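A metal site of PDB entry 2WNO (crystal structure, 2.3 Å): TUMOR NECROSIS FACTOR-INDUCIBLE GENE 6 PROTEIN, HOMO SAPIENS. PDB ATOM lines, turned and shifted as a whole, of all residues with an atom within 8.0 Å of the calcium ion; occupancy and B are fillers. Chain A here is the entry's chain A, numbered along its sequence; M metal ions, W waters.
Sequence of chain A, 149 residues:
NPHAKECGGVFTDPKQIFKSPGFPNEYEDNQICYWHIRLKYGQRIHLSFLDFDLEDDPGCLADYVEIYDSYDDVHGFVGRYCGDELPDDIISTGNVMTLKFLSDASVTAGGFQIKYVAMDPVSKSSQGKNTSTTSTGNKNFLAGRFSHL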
ATOM      1  N   TYR A  27      23.087  12.669  25.484  1.00  0.00           N
ATOM      2  CA  TYR A  27      23.984  13.251  24.489  1.00  0.00           C
ATOM      3  C   TYR A  27      25.349  13.477  25.133  1.00  0.00           C
ATOM      4  O   TYR A  27      25.499  13.408  26.357  1.00  0.00           O
ATOM      5  CB  TYR A  27      23.407  14.545  23.885  1.00  0.00           C
ATOM      6  CG  TYR A  27      23.078  15.670  24.853  1.00  0.00           C
ATOM      7  CD1 TYR A  27      24.063  16.561  25.285  1.00  0.00           C
ATOM      8  CD2 TYR A  27      21.765  15.871  25.303  1.00  0.00           C
ATOM      9  CE1 TYR A  27      23.755  17.604  26.156  1.00  0.00           C
ATOM     10  CE2 TYR A  27      21.442  16.914  26.182  1.00  0.00           C
ATOM     11  CZ  TYR A  27      22.456  17.776  26.606  1.00  0.00           C
ATOM     12  OH  TYR A  27      22.169  18.810  27.481  1.00  0.00           O
ATOM     13  N   GLU A  28      26.360  13.716  24.299  1.00  0.00           N
ATOM     14  CA  GLU A  28      27.695  14.024  24.791  1.00  0.00           C
ATOM     15  C   GLU A  28      27.962  15.530  24.804  1.00  0.00           C
ATOM     16  O   GLU A  28      27.187  16.327  24.248  1.00  0.00           O
ATOM     17  CB  GLU A  28      28.751  13.282  23.983  1.00  0.00           C
ATOM     18  CG  GLU A  28      28.726  11.765  24.173  1.00  0.00           C
ATOM     19  CD  GLU A  28      29.848  11.076  23.446  1.00  0.00           C
ATOM     20  OE1 GLU A  28      29.577  10.482  22.381  1.00  0.00           O
ATOM     21  OE2 GLU A  28      31.006  11.143  23.927  1.00  0.00           O
ATOM     22  N   ASP A  29      29.062  15.922  25.452  1.00  0.00           N
ATOM     23  CA  ASP A  29      29.517  17.301  25.458  1.00  0.00           C
ATOM     24  C   ASP A  29      30.043  17.697  24.090  1.00  0.00           C
ATOM     25  O   ASP A  29      30.467  16.833  23.303  1.00  0.00           O
ATOM     26  CB  ASP A  29      30.627  17.503  26.509  1.00  0.00           C
ATOM     27  CG  ASP A  29      30.134  17.264  27.932  1.00  0.00           C
ATOM     28  OD1 ASP A  29      30.824  16.540  28.683  1.00  0.00           O
ATOM     29  OD2 ASP A  29      29.064  17.799  28.314  1.00  0.00           O
ATOM     30  N   ASN A  30      30.011  19.006  23.804  1.00  0.00           N
ATOM     31  CA  ASN A  30      30.603  19.581  22.592  1.00  0.00           C
ATOM     32  C   ASN A  30      29.963  19.083  21.308  1.00  0.00           C
ATOM     33  O   ASN A  30      30.607  19.017  20.263  1.00  0.00           O
ATOM     34  CB  ASN A  30      32.129  19.346  22.551  1.00  0.00           C
ATOM     35  CG  ASN A  30      32.822  19.796  23.810  1.00  0.00           C
ATOM     36  OD1 ASN A  30      32.716  20.957  24.212  1.00  0.00           O
ATOM     37  ND2 ASN A  30      33.552  18.884  24.446  1.00  0.00           N
ATOM     38  N   GLN A  31      28.676  18.741  21.397  1.00  0.00           N
ATOM     39  CA  GLN A  31      27.924  18.274  20.248  1.00  0.00           C
ATOM     40  C   GLN A  31      27.281  19.444  19.503  1.00  0.00           C
ATOM     41  O   GLN A  31      26.766  20.375  20.114  1.00  0.00           O
ATOM     42  CB  GLN A  31      26.873  17.241  20.690  1.00  0.00           C
ATOM     43  CG  GLN A  31      26.149  16.517  19.539  1.00  0.00           C
ATOM     44  CD  GLN A  31      27.091  15.708  18.669  1.00  0.00           C
ATOM     45  OE1 GLN A  31      27.942  14.977  19.186  1.00  0.00           O
ATOM     46  NE2 GLN A  31      26.940  15.822  17.357  1.00  0.00           N
ATOM     47  N   LEU A  54      17.343  18.778  27.954  1.00  0.00           N
ATOM     48  CA  LEU A  54      18.685  19.345  27.871  1.00  0.00           C
ATOM     49  C   LEU A  54      19.097  19.991  29.185  1.00  0.00           C
ATOM     50  O   LEU A  54      18.282  20.187  30.076  1.00  0.00           O
ATOM     51  CB  LEU A  54      18.797  20.383  26.743  1.00  0.00           C
ATOM     52  CG  LEU A  54      18.438  20.124  25.276  1.00  0.00           C
ATOM     53  CD1 LEU A  54      19.286  21.024  24.439  1.00  0.00           C
ATOM     54  CD2 LEU A  54      18.586  18.685  24.801  1.00  0.00           C
ATOM     55  N   GLU A  55      20.375  20.339  29.290  1.00  0.00           N
ATOM     56  CA  GLU A  55      20.836  21.148  30.406  1.00  0.00           C
ATOM     57  C   GLU A  55      20.006  22.429  30.488  1.00  0.00           C
ATOM     58  O   GLU A  55      19.690  23.036  29.462  1.00  0.00           O
ATOM     59  CB  GLU A  55      22.308  21.501  30.223  1.00  0.00           C
ATOM     60  CG  GLU A  55      22.870  22.411  31.300  1.00  0.00           C
ATOM     61  CD  GLU A  55      24.312  22.734  31.076  1.00  0.00           C
ATOM     62  OE1 GLU A  55      24.895  22.266  30.078  1.00  0.00           O
ATOM     63  OE2 GLU A  55      24.883  23.472  31.910  1.00  0.00           O
ATOM     64  N   ASP A  56      19.644  22.829  31.699  1.00  0.00           N
ATOM     65  CA  ASP A  56      18.844  24.023  31.900  1.00  0.00           C
ATOM     66  C   ASP A  56      19.677  25.202  32.415  1.00  0.00           C
ATOM     67  O   ASP A  56      20.531  25.040  33.301  1.00  0.00           O
ATOM     68  CB  ASP A  56      17.682  23.726  32.861  1.00  0.00           C
ATOM     69  CG  ASP A  56      16.497  24.666  32.669  1.00  0.00           C
ATOM     70  OD1 ASP A  56      16.447  25.391  31.649  1.00  0.00           O
ATOM     71  OD2 ASP A  56      15.604  24.669  33.533  1.00  0.00           O
ATOM     72  N   ASP A  57      19.442  26.374  31.836  1.00  0.00           N
ATOM     73  CA  ASP A  57      19.850  27.635  32.447  1.00  0.00           C
ATOM     74  C   ASP A  57      18.993  28.790  31.903  1.00  0.00           C
ATOM     75  O   ASP A  57      18.382  28.644  30.828  1.00  0.00           O
ATOM     76  CB  ASP A  57      21.371  27.891  32.355  1.00  0.00           C
ATOM     77  CG  ASP A  57      21.833  28.241  30.969  1.00  0.00           C
ATOM     78  OD1 ASP A  57      21.728  29.440  30.615  1.00  0.00           O
ATOM     79  OD2 ASP A  57      22.325  27.336  30.264  1.00  0.00           O
ATOM     80  N   LEU A  61      22.143  29.216  27.555  1.00  0.00           N
ATOM     81  CA  LEU A  61      23.432  29.635  27.044  1.00  0.00           C
ATOM     82  C   LEU A  61      24.382  28.457  26.896  1.00  0.00           C
ATOM     83  O   LEU A  61      25.370  28.536  26.163  1.00  0.00           O
ATOM     84  CB  LEU A  61      24.055  30.682  27.963  1.00  0.00           C
ATOM     85  CG  LEU A  61      23.232  31.912  28.359  1.00  0.00           C
ATOM     86  CD1 LEU A  61      24.008  32.714  29.375  1.00  0.00           C
ATOM     87  CD2 LEU A  61      22.873  32.763  27.145  1.00  0.00           C
ATOM     88  N   ALA A  62      24.078  27.376  27.599  1.00  0.00           N
ATOM     89  CA  ALA A  62      24.907  26.166  27.577  1.00  0.00           C
ATOM     90  C   ALA A  62      24.471  25.206  26.470  1.00  0.00           C
ATOM     91  O   ALA A  62      25.138  25.108  25.446  1.00  0.00           O
ATOM     92  CB  ALA A  62      24.890  25.488  28.948  1.00  0.00           C
ATOM     93  N   ASP A  63      23.367  24.486  26.689  1.00  0.00           N
ATOM     94  CA  ASP A  63      22.838  23.558  25.699  1.00  0.00           C
ATOM     95  C   ASP A  63      21.497  24.026  25.208  1.00  0.00           C
ATOM     96  O   ASP A  63      20.692  24.534  25.991  1.00  0.00           O
ATOM     97  CB  ASP A  63      22.651  22.156  26.299  1.00  0.00           C
ATOM     98  CG  ASP A  63      23.934  21.572  26.828  1.00  0.00           C
ATOM     99  OD1 ASP A  63      23.886  20.468  27.397  1.00  0.00           O
ATOM    100  OD2 ASP A  63      24.997  22.220  26.685  1.00  0.00           O
ATOM    101  N   TYR A  64      21.255  23.857  23.908  1.00  0.00           N
ATOM    102  CA  TYR A  64      19.997  24.284  23.316  1.00  0.00           C
ATOM    103  C   TYR A  64      19.675  23.571  22.002  1.00  0.00           C
ATOM    104  O   TYR A  64      20.558  23.034  21.325  1.00  0.00           O
ATOM    105  CB  TYR A  64      19.991  25.798  23.099  1.00  0.00           C
ATOM    106  CG  TYR A  64      21.136  26.304  22.249  1.00  0.00           C
ATOM    107  CD1 TYR A  64      21.039  26.326  20.856  1.00  0.00           C
ATOM    108  CD2 TYR A  64      22.308  26.770  22.848  1.00  0.00           C
ATOM    109  CE1 TYR A  64      22.088  26.792  20.075  1.00  0.00           C
ATOM    110  CE2 TYR A  64      23.374  27.250  22.062  1.00  0.00           C
ATOM    111  CZ  TYR A  64      23.244  27.258  20.681  1.00  0.00           C
ATOM    112  OH  TYR A  64      24.277  27.710  19.905  1.00  0.00           O
ATOM    113  N   PHE A 101      21.156  21.918  17.118  1.00  0.00           N
ATOM    114  CA  PHE A 101      21.433  21.475  18.461  1.00  0.00           C
ATOM    115  C   PHE A 101      22.884  21.755  18.800  1.00  0.00           C
ATOM    116  O   PHE A 101      23.786  21.480  18.000  1.00  0.00           O
ATOM    117  CB  PHE A 101      21.118  19.979  18.624  1.00  0.00           C
ATOM    118  CG  PHE A 101      21.627  19.377  19.916  1.00  0.00           C
ATOM    119  CD1 PHE A 101      21.230  19.868  21.151  1.00  0.00           C
ATOM    120  CD2 PHE A 101      22.510  18.296  19.878  1.00  0.00           C
ATOM    121  CE1 PHE A 101      21.705  19.308  22.337  1.00  0.00           C
ATOM    122  CE2 PHE A 101      22.971  17.722  21.060  1.00  0.00           C
ATOM    123  CZ  PHE A 101      22.569  18.236  22.286  1.00  0.00           C
ATOM    124  N   LEU A 102      23.108  22.315  19.984  1.00  0.00           N
ATOM    125  CA  LEU A 102      24.460  22.478  20.495  1.00  0.00           C
ATOM    126  C   LEU A 102      24.512  22.154  21.990  1.00  0.00           C
ATOM    127  O   LEU A 102      23.692  22.635  22.767  1.00  0.00           O
ATOM    128  CB  LEU A 102      24.982  23.896  20.212  1.00  0.00           C
ATOM    129  CG  LEU A 102      26.464  24.186  20.506  1.00  0.00           C
ATOM    130  CD1 LEU A 102      27.029  25.181  19.488  1.00  0.00           C
ATOM    131  CD2 LEU A 102      26.681  24.719  21.933  1.00  0.00           C
ATOM    132  N   SER A 103      25.479  21.328  22.366  1.00  0.00           N
ATOM    133  CA  SER A 103      25.847  21.160  23.768  1.00  0.00           C
ATOM    134  C   SER A 103      27.227  21.759  24.014  1.00  0.00           C
ATOM    135  O   SER A 103      28.096  21.693  23.148  1.00  0.00           O
ATOM    136  CB  SER A 103      25.799  19.695  24.195  1.00  0.00           C
ATOM    137  OG  SER A 103      26.719  18.905  23.477  1.00  0.00           O
ATOM    138  N   ASP A 104      27.433  22.357  25.188  1.00  0.00           N
ATOM    139  CA  ASP A 104      28.737  22.910  25.547  1.00  0.00           C
ATOM    140  C   ASP A 104      29.670  21.870  26.180  1.00  0.00           C
ATOM    141  O   ASP A 104      29.469  20.666  25.998  1.00  0.00           O
ATOM    142  CB  ASP A 104      28.587  24.174  26.423  1.00  0.00           C
ATOM    143  CG  ASP A 104      28.041  23.884  27.809  1.00  0.00           C
ATOM    144  OD1 ASP A 104      28.149  24.761  28.686  1.00  0.00           O
ATOM    145  OD2 ASP A 104      27.511  22.779  28.042  1.00  0.00           O
ATOM    146  N   ALA A 105      30.676  22.319  26.918  1.00  0.00           N
ATOM    147  CA  ALA A 105      31.773  21.483  27.401  1.00  0.00           C
ATOM    148  C   ALA A 105      31.454  20.587  28.594  1.00  0.00           C
ATOM    149  O   ALA A 105      32.175  19.626  28.863  1.00  0.00           O
ATOM    150  CB  ALA A 105      32.984  22.352  27.703  1.00  0.00           C
ATOM    151  N   SER A 106      30.384  20.906  29.312  1.00  0.00           N
ATOM    152  CA  SER A 106      30.027  20.166  30.524  1.00  0.00           C
ATOM    153  C   SER A 106      28.528  20.002  30.681  1.00  0.00           C
ATOM    154  O   SER A 106      27.749  20.796  30.145  1.00  0.00           O
ATOM    155  CB  SER A 106      30.610  20.864  31.756  1.00  0.00           C
ATOM    156  OG  SER A 106      30.167  22.209  31.842  1.00  0.00           O
ATOM    157  N   VAL A 107      28.123  18.968  31.430  1.00  0.00           N
ATOM    158  CA  VAL A 107      26.730  18.685  31.781  1.00  0.00           C
ATOM    159  C   VAL A 107      25.894  18.233  30.585  1.00  0.00           C
ATOM    160  O   VAL A 107      25.696  18.979  29.619  1.00  0.00           O
ATOM    161  CB  VAL A 107      26.001  19.875  32.489  1.00  0.00           C
ATOM    162  CG1 VAL A 107      24.624  19.431  33.000  1.00  0.00           C
ATOM    163  CG2 VAL A 107      26.846  20.439  33.637  1.00  0.00           C
ATOM    164  N   THR A 108      25.403  17.003  30.659  1.00  0.00           N
ATOM    165  CA  THR A 108      24.602  16.444  29.582  1.00  0.00           C
ATOM    166  C   THR A 108      23.252  16.069  30.157  1.00  0.00           C
ATOM    167  O   THR A 108      23.056  16.120  31.375  1.00  0.00           O
ATOM    168  CB  THR A 108      25.295  15.226  28.935  1.00  0.00           C
ATOM    169  OG1 THR A 108      25.531  14.220  29.922  1.00  0.00           O
ATOM    170  CG2 THR A 108      26.632  15.627  28.319  1.00  0.00           C
ATOM    171  N   ALA A 109      22.322  15.705  29.280  1.00  0.00           N
ATOM    172  CA  ALA A 109      20.993  15.283  29.701  1.00  0.00           C
ATOM    173  C   ALA A 109      20.449  14.273  28.689  1.00  0.00           C
ATOM    174  O   ALA A 109      21.159  13.899  27.768  1.00  0.00           O
ATOM    175  CB  ALA A 109      20.073  16.502  29.859  1.00  0.00           C
HETATM  176 CA    CA M   1      26.090  21.017  28.566  1.00  0.00          CA
HETATM  177  O   HOH W   1      27.397  19.541  27.555  1.00  0.00           O
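The backbone NH of Val 107 lies within hydrogen-bond range of the side-chain carboxylate of Asp 29 (3.5 Å).
The backbone carbonyl oxygen of Asp 104 is in hydrogen-bond range of the backbone NH of Asn 30.
The backbone NH of Glu 55 sits at hydrogen-bond distance from the side-chain hydroxyl of Tyr 27 (3.0 Å).
Of the 22 residues printed, 5 come within 4 Å of the calcium ion.
The calcium ion is bound by water W1 (2.2 Å), the side-chain carboxylate (OE1) of Glu 55 (2.3 Å), the backbone carbonyl oxygen (O) of Ser 106 (2.3 Å), the side-chain carboxylate (OD2) of Asp 104 (2.3 Å), the backbone carbonyl oxygen (O) of Val 107 (2.3 Å), the side-chain carboxylate (OD2) of Asp 63 (2.5 Å) and the side-chain carboxylate (OD1) of Asp 63 (2.6 Å).
Water W1 bridges the side-chain carboxylate of Asp 29 and the backbone carbonyl oxygen of Asp 104.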
